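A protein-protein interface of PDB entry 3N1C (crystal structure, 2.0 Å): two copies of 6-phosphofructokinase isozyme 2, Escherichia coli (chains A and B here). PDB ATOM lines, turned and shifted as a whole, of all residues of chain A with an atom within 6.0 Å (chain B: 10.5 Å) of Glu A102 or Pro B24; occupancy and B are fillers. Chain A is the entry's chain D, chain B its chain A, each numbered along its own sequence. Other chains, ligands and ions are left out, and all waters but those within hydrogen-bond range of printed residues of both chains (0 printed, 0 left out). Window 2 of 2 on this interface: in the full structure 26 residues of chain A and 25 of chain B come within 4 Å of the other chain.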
ATOM      1  N   ILE A  22     -16.530  31.267 -21.323  1.00  0.00           N
ATOM      2  CA  ILE A  22     -17.351  32.397 -21.727  1.00  0.00           C
ATOM      3  C   ILE A  22     -17.318  33.528 -20.703  1.00  0.00           C
ATOM      4  O   ILE A  22     -17.548  33.317 -19.512  1.00  0.00           O
ATOM      5  CB  ILE A  22     -18.807  31.968 -21.990  1.00  0.00           C
ATOM      6  CG1 ILE A  22     -19.634  33.164 -22.468  1.00  0.00           C
ATOM      7  CG2 ILE A  22     -19.405  31.335 -20.743  1.00  0.00           C
ATOM      8  CD1 ILE A  22     -20.908  32.780 -23.192  1.00  0.00           C
ATOM      9  N   VAL A  95     -22.626  27.693 -29.354  1.00  0.00           N
ATOM     10  CA  VAL A  95     -21.305  27.724 -28.751  1.00  0.00           C
ATOM     11  C   VAL A  95     -21.263  26.776 -27.573  1.00  0.00           C
ATOM     12  O   VAL A  95     -21.961  26.982 -26.585  1.00  0.00           O
ATOM     13  CB  VAL A  95     -20.939  29.125 -28.250  1.00  0.00           C
ATOM     14  CG1 VAL A  95     -19.501  29.142 -27.738  1.00  0.00           C
ATOM     15  CG2 VAL A  95     -21.136  30.165 -29.347  1.00  0.00           C
ATOM     16  N   HIS A  96     -20.452  25.733 -27.684  1.00  0.00           N
ATOM     17  CA  HIS A  96     -20.219  24.846 -26.555  1.00  0.00           C
ATOM     18  C   HIS A  96     -19.013  25.326 -25.763  1.00  0.00           C
ATOM     19  O   HIS A  96     -17.913  25.468 -26.312  1.00  0.00           O
ATOM     20  CB  HIS A  96     -19.996  23.411 -27.022  1.00  0.00           C
ATOM     21  CG  HIS A  96     -19.579  22.484 -25.923  1.00  0.00           C
ATOM     22  ND1 HIS A  96     -20.455  22.039 -24.953  1.00  0.00           N
ATOM     23  CD2 HIS A  96     -18.381  21.927 -25.629  1.00  0.00           C
ATOM     24  CE1 HIS A  96     -19.815  21.242 -24.118  1.00  0.00           C
ATOM     25  NE2 HIS A  96     -18.554  21.157 -24.504  1.00  0.00           N
ATOM     26  N   VAL A  97     -19.218  25.572 -24.474  1.00  0.00           N
ATOM     27  CA  VAL A  97     -18.140  26.028 -23.609  1.00  0.00           C
ATOM     28  C   VAL A  97     -17.522  24.849 -22.860  1.00  0.00           C
ATOM     29  O   VAL A  97     -18.182  24.219 -22.032  1.00  0.00           O
ATOM     30  CB  VAL A  97     -18.643  27.063 -22.592  1.00  0.00           C
ATOM     31  CG1 VAL A  97     -17.481  27.616 -21.787  1.00  0.00           C
ATOM     32  CG2 VAL A  97     -19.395  28.189 -23.301  1.00  0.00           C
ATOM     33  N   GLU A  98     -16.259  24.554 -23.157  1.00  0.00           N
ATOM     34  CA  GLU A  98     -15.572  23.392 -22.588  1.00  0.00           C
ATOM     35  C   GLU A  98     -15.496  23.399 -21.062  1.00  0.00           C
ATOM     36  O   GLU A  98     -15.724  22.375 -20.419  1.00  0.00           O
ATOM     37  CB  GLU A  98     -14.164  23.260 -23.173  1.00  0.00           C
ATOM     38  CG  GLU A  98     -14.119  22.609 -24.542  1.00  0.00           C
ATOM     39  CD  GLU A  98     -12.767  22.763 -25.217  1.00  0.00           C
ATOM     40  OE1 GLU A  98     -12.445  21.940 -26.102  1.00  0.00           O
ATOM     41  OE2 GLU A  98     -12.025  23.707 -24.865  1.00  0.00           O
ATOM     42  N   ALA A  99     -15.171  24.550 -20.486  1.00  0.00           N
ATOM     43  CA  ALA A  99     -14.983  24.650 -19.044  1.00  0.00           C
ATOM     44  C   ALA A  99     -16.224  24.224 -18.266  1.00  0.00           C
ATOM     45  O   ALA A  99     -16.121  23.574 -17.226  1.00  0.00           O
ATOM     46  CB  ALA A  99     -14.582  26.070 -18.661  1.00  0.00           C
ATOM     47  N   SER A 100     -17.395  24.590 -18.779  1.00  0.00           N
ATOM     48  CA  SER A 100     -18.647  24.388 -18.061  1.00  0.00           C
ATOM     49  C   SER A 100     -19.519  23.288 -18.661  1.00  0.00           C
ATOM     50  O   SER A 100     -20.477  22.836 -18.030  1.00  0.00           O
ATOM     51  CB  SER A 100     -19.440  25.696 -18.017  1.00  0.00           C
ATOM     52  OG  SER A 100     -19.703  26.176 -19.326  1.00  0.00           O
ATOM     53  N   GLY A 101     -19.192  22.862 -19.878  1.00  0.00           N
ATOM     54  CA  GLY A 101     -20.005  21.891 -20.586  1.00  0.00           C
ATOM     55  C   GLY A 101     -21.317  22.496 -21.053  1.00  0.00           C
ATOM     56  O   GLY A 101     -22.178  21.798 -21.587  1.00  0.00           O
ATOM     57  N   GLU A 102     -21.460  23.803 -20.858  1.00  0.00           N
ATOM     58  CA  GLU A 102     -22.675  24.518 -21.229  1.00  0.00           C
ATOM     59  C   GLU A 102     -22.713  24.811 -22.719  1.00  0.00           C
ATOM     60  O   GLU A 102     -21.669  24.936 -23.355  1.00  0.00           O
ATOM     61  CB  GLU A 102     -22.758  25.843 -20.466  1.00  0.00           C
ATOM     62  CG  GLU A 102     -22.984  25.708 -18.974  1.00  0.00           C
ATOM     63  CD  GLU A 102     -22.939  27.047 -18.262  1.00  0.00           C
ATOM     64  OE1 GLU A 102     -23.596  27.182 -17.209  1.00  0.00           O
ATOM     65  OE2 GLU A 102     -22.250  27.967 -18.759  1.00  0.00           O
ATOM     66  N   GLN A 103     -23.915  24.934 -23.276  1.00  0.00           N
ATOM     67  CA  GLN A 103     -24.054  25.369 -24.662  1.00  0.00           C
ATOM     68  C   GLN A 103     -24.923  26.614 -24.774  1.00  0.00           C
ATOM     69  O   GLN A 103     -25.978  26.704 -24.145  1.00  0.00           O
ATOM     70  CB  GLN A 103     -24.618  24.259 -25.548  1.00  0.00           C
ATOM     71  CG  GLN A 103     -24.462  24.559 -27.034  1.00  0.00           C
ATOM     72  CD  GLN A 103     -24.974  23.441 -27.919  1.00  0.00           C
ATOM     73  OE1 GLN A 103     -24.578  23.316 -29.080  1.00  0.00           O
ATOM     74  NE2 GLN A 103     -25.858  22.619 -27.372  1.00  0.00           N
ATOM     75  N   TYR A 104     -24.472  27.575 -25.572  1.00  0.00           N
ATOM     76  CA  TYR A 104     -25.219  28.814 -25.777  1.00  0.00           C
ATOM     77  C   TYR A 104     -25.736  28.885 -27.203  1.00  0.00           C
ATOM     78  O   TYR A 104     -25.032  28.518 -28.142  1.00  0.00           O
ATOM     79  CB  TYR A 104     -24.346  30.029 -25.454  1.00  0.00           C
ATOM     80  CG  TYR A 104     -24.044  30.161 -23.978  1.00  0.00           C
ATOM     81  CD1 TYR A 104     -23.089  29.354 -23.370  1.00  0.00           C
ATOM     82  CD2 TYR A 104     -24.726  31.083 -23.188  1.00  0.00           C
ATOM     83  CE1 TYR A 104     -22.817  29.463 -22.023  1.00  0.00           C
ATOM     84  CE2 TYR A 104     -24.458  31.200 -21.836  1.00  0.00           C
ATOM     85  CZ  TYR A 104     -23.502  30.388 -21.260  1.00  0.00           C
ATOM     86  OH  TYR A 104     -23.227  30.498 -19.916  1.00  0.00           O
ATOM     87  N   GLN B  21     -31.303  38.656 -23.004  1.00  0.00           N
ATOM     88  CA  GLN B  21     -30.712  37.895 -21.907  1.00  0.00           C
ATOM     89  C   GLN B  21     -29.612  36.958 -22.406  1.00  0.00           C
ATOM     90  O   GLN B  21     -29.603  36.572 -23.576  1.00  0.00           O
ATOM     91  CB  GLN B  21     -31.792  37.055 -21.212  1.00  0.00           C
ATOM     92  CG  GLN B  21     -33.107  37.784 -20.945  1.00  0.00           C
ATOM     93  CD  GLN B  21     -33.090  38.559 -19.643  1.00  0.00           C
ATOM     94  OE1 GLN B  21     -33.833  39.528 -19.474  1.00  0.00           O
ATOM     95  NE2 GLN B  21     -32.237  38.139 -18.715  1.00  0.00           N
ATOM     96  N   ILE B  22     -28.697  36.584 -21.514  1.00  0.00           N
ATOM     97  CA  ILE B  22     -27.739  35.517 -21.813  1.00  0.00           C
ATOM     98  C   ILE B  22     -27.704  34.437 -20.724  1.00  0.00           C
ATOM     99  O   ILE B  22     -27.444  34.713 -19.553  1.00  0.00           O
ATOM    100  CB  ILE B  22     -26.321  36.056 -22.087  1.00  0.00           C
ATOM    101  CG1 ILE B  22     -25.441  34.956 -22.693  1.00  0.00           C
ATOM    102  CG2 ILE B  22     -25.701  36.626 -20.824  1.00  0.00           C
ATOM    103  CD1 ILE B  22     -24.167  35.473 -23.332  1.00  0.00           C
ATOM    104  N   TYR B  23     -27.986  33.205 -21.131  1.00  0.00           N
ATOM    105  CA  TYR B  23     -27.971  32.051 -20.243  1.00  0.00           C
ATOM    106  C   TYR B  23     -27.846  30.802 -21.110  1.00  0.00           C
ATOM    107  O   TYR B  23     -28.158  30.844 -22.302  1.00  0.00           O
ATOM    108  CB  TYR B  23     -29.239  31.999 -19.380  1.00  0.00           C
ATOM    109  CG  TYR B  23     -30.527  31.962 -20.173  1.00  0.00           C
ATOM    110  CD1 TYR B  23     -31.120  30.754 -20.517  1.00  0.00           C
ATOM    111  CD2 TYR B  23     -31.149  33.134 -20.582  1.00  0.00           C
ATOM    112  CE1 TYR B  23     -32.295  30.713 -21.243  1.00  0.00           C
ATOM    113  CE2 TYR B  23     -32.323  33.103 -21.313  1.00  0.00           C
ATOM    114  CZ  TYR B  23     -32.889  31.892 -21.640  1.00  0.00           C
ATOM    115  OH  TYR B  23     -34.056  31.857 -22.368  1.00  0.00           O
ATOM    116  N   PRO B  24     -27.366  29.695 -20.526  1.00  0.00           N
ATOM    117  CA  PRO B  24     -27.132  28.455 -21.275  1.00  0.00           C
ATOM    118  C   PRO B  24     -28.413  27.752 -21.721  1.00  0.00           C
ATOM    119  O   PRO B  24     -29.489  27.989 -21.166  1.00  0.00           O
ATOM    120  CB  PRO B  24     -26.388  27.576 -20.258  1.00  0.00           C
ATOM    121  CG  PRO B  24     -26.777  28.157 -18.912  1.00  0.00           C
ATOM    122  CD  PRO B  24     -26.784  29.623 -19.174  1.00  0.00           C
ATOM    123  N   GLU B  25     -28.280  26.900 -22.733  1.00  0.00           N
ATOM    124  CA  GLU B  25     -29.343  25.987 -23.141  1.00  0.00           C
ATOM    125  C   GLU B  25     -30.498  26.622 -23.914  1.00  0.00           C
ATOM    126  O   GLU B  25     -30.887  26.123 -24.970  1.00  0.00           O
ATOM    127  CB  GLU B  25     -29.867  25.206 -21.932  1.00  0.00           C
ATOM    128  CG  GLU B  25     -29.260  23.817 -21.780  1.00  0.00           C
ATOM    129  CD  GLU B  25     -27.859  23.711 -22.357  1.00  0.00           C
ATOM    130  OE1 GLU B  25     -26.902  24.195 -21.711  1.00  0.00           O
ATOM    131  OE2 GLU B  25     -27.716  23.125 -23.454  1.00  0.00           O
ATOM    132  N   GLY B  26     -31.049  27.711 -23.395  1.00  0.00           N
ATOM    133  CA  GLY B  26     -32.234  28.306 -23.991  1.00  0.00           C
ATOM    134  C   GLY B  26     -31.952  29.005 -25.306  1.00  0.00           C
ATOM    135  O   GLY B  26     -30.830  29.441 -25.559  1.00  0.00           O
ATOM    136  N   LYS B  27     -32.973  29.102 -26.152  1.00  0.00           N
ATOM    137  CA  LYS B  27     -32.847  29.824 -27.411  1.00  0.00           C
ATOM    138  C   LYS B  27     -32.816  31.326 -27.157  1.00  0.00           C
ATOM    139  O   LYS B  27     -33.818  31.924 -26.758  1.00  0.00           O
ATOM    140  CB  LYS B  27     -33.983  29.458 -28.369  1.00  0.00           C
ATOM    141  CG  LYS B  27     -33.877  28.046 -28.923  1.00  0.00           C
ATOM    142  CD  LYS B  27     -34.973  27.742 -29.933  1.00  0.00           C
ATOM    143  CE  LYS B  27     -34.942  26.269 -30.325  1.00  0.00           C
ATOM    144  NZ  LYS B  27     -36.069  25.897 -31.223  1.00  0.00           N
ATOM    145  N   LEU B  28     -31.652  31.930 -27.373  1.00  0.00           N
ATOM    146  CA  LEU B  28     -31.494  33.365 -27.189  1.00  0.00           C
ATOM    147  C   LEU B  28     -31.902  34.106 -28.460  1.00  0.00           C
ATOM    148  O   LEU B  28     -31.216  34.033 -29.479  1.00  0.00           O
ATOM    149  CB  LEU B  28     -30.054  33.700 -26.797  1.00  0.00           C
ATOM    150  CG  LEU B  28     -29.510  32.918 -25.593  1.00  0.00           C
ATOM    151  CD1 LEU B  28     -28.070  33.322 -25.285  1.00  0.00           C
ATOM    152  CD2 LEU B  28     -30.396  33.114 -24.371  1.00  0.00           C
ATOM    153  N   TYR B 104     -20.426  40.184 -25.772  1.00  0.00           N
ATOM    154  CA  TYR B 104     -19.702  38.933 -25.954  1.00  0.00           C
ATOM    155  C   TYR B 104     -19.153  38.808 -27.366  1.00  0.00           C
ATOM    156  O   TYR B 104     -19.840  39.117 -28.342  1.00  0.00           O
ATOM    157  CB  TYR B 104     -20.595  37.746 -25.604  1.00  0.00           C
ATOM    158  CG  TYR B 104     -20.933  37.694 -24.136  1.00  0.00           C
ATOM    159  CD1 TYR B 104     -22.047  38.357 -23.637  1.00  0.00           C
ATOM    160  CD2 TYR B 104     -20.127  37.002 -23.244  1.00  0.00           C
ATOM    161  CE1 TYR B 104     -22.353  38.326 -22.287  1.00  0.00           C
ATOM    162  CE2 TYR B 104     -20.425  36.964 -21.892  1.00  0.00           C
ATOM    163  CZ  TYR B 104     -21.537  37.626 -21.418  1.00  0.00           C
ATOM    164  OH  TYR B 104     -21.834  37.583 -20.071  1.00  0.00           O
ATOM    165  N   PHE B 106     -17.345  36.410 -30.151  1.00  0.00           N
ATOM    166  CA  PHE B 106     -16.997  35.077 -30.618  1.00  0.00           C
ATOM    167  C   PHE B 106     -16.138  35.151 -31.875  1.00  0.00           C
ATOM    168  O   PHE B 106     -16.592  35.552 -32.949  1.00  0.00           O
ATOM    169  CB  PHE B 106     -18.261  34.243 -30.822  1.00  0.00           C
ATOM    170  CG  PHE B 106     -19.093  34.117 -29.575  1.00  0.00           C
ATOM    171  CD1 PHE B 106     -20.196  34.929 -29.374  1.00  0.00           C
ATOM    172  CD2 PHE B 106     -18.747  33.206 -28.588  1.00  0.00           C
ATOM    173  CE1 PHE B 106     -20.943  34.823 -28.221  1.00  0.00           C
ATOM    174  CE2 PHE B 106     -19.487  33.100 -27.435  1.00  0.00           C
ATOM    175  CZ  PHE B 106     -20.591  33.905 -27.253  1.00  0.00           C
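Of the printed residues of chain B, Ile A22 touches Tyr B104 (3.9 Å). No residue of chain B comes within 4 Å of His A96. Glu A98 touches none of the printed residues of chain B. No residue of chain B comes within 4 Å of Ser A100. No residue of chain B comes within 4 Å of Gly A101. Glu A102 touches one residue of chain B. Printed residues of chain B within 4 Å of Gln A103: Pro B24 (3.6 Å) and Glu B25 (2.7 Å). Pro B24 touches three residues of chain A. Of the printed residues of chain A, Glu B25 touches Gln A103 (2.7 Å). The nearest printed residue of chain A that does not touch Tyr B104 is Tyr A104 (7.0 Å).
Ile A22 touches Tyr B104. Phe B106 touches Val A95. Pro B24 touches Glu A102. Pro B24 touches Gln A103. Ile B22 touches Tyr A104. C of Tyr B23 touches CE2 of Tyr A104, 3.5 Å away. CE2 of Tyr A104 touches N of Pro B24, at 3.5 Å.
Of the 10 printed residues of chain B, 6 touch a printed residue of chain A. Hydrophobic or aromatic side chains of chain B that line the printed part of chain A: Ile B22, Pro B24, Tyr B104 and Phe B106.
Ile A22 touches Tyr B104, and with the chains exchanged Tyr A104 touches Ile B22. Positions printed for both chains: 22 and 104. Of the 8 pairs that touch across the chains among the printed residues, 2 have their exchanged pair printed and touching as well.
O of Val A95 lies within hydrogen-bond range of N of Tyr A104 (2.8 Å). N of Val A97 sits at hydrogen-bond distance from O of Glu A102, at 2.8 Å. The side-chain hydroxyl (OG) of Ser A100 is in hydrogen-bond range of the side-chain carboxylate (OE2) of Glu A102, 3.2 Å away. OH of Tyr A104 lies within hydrogen-bond range of OE2 of Glu A102, 2.9 Å away.
The backbone NH of Glu B25 lies within hydrogen-bond range of the backbone carbonyl oxygen of Gln A103.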
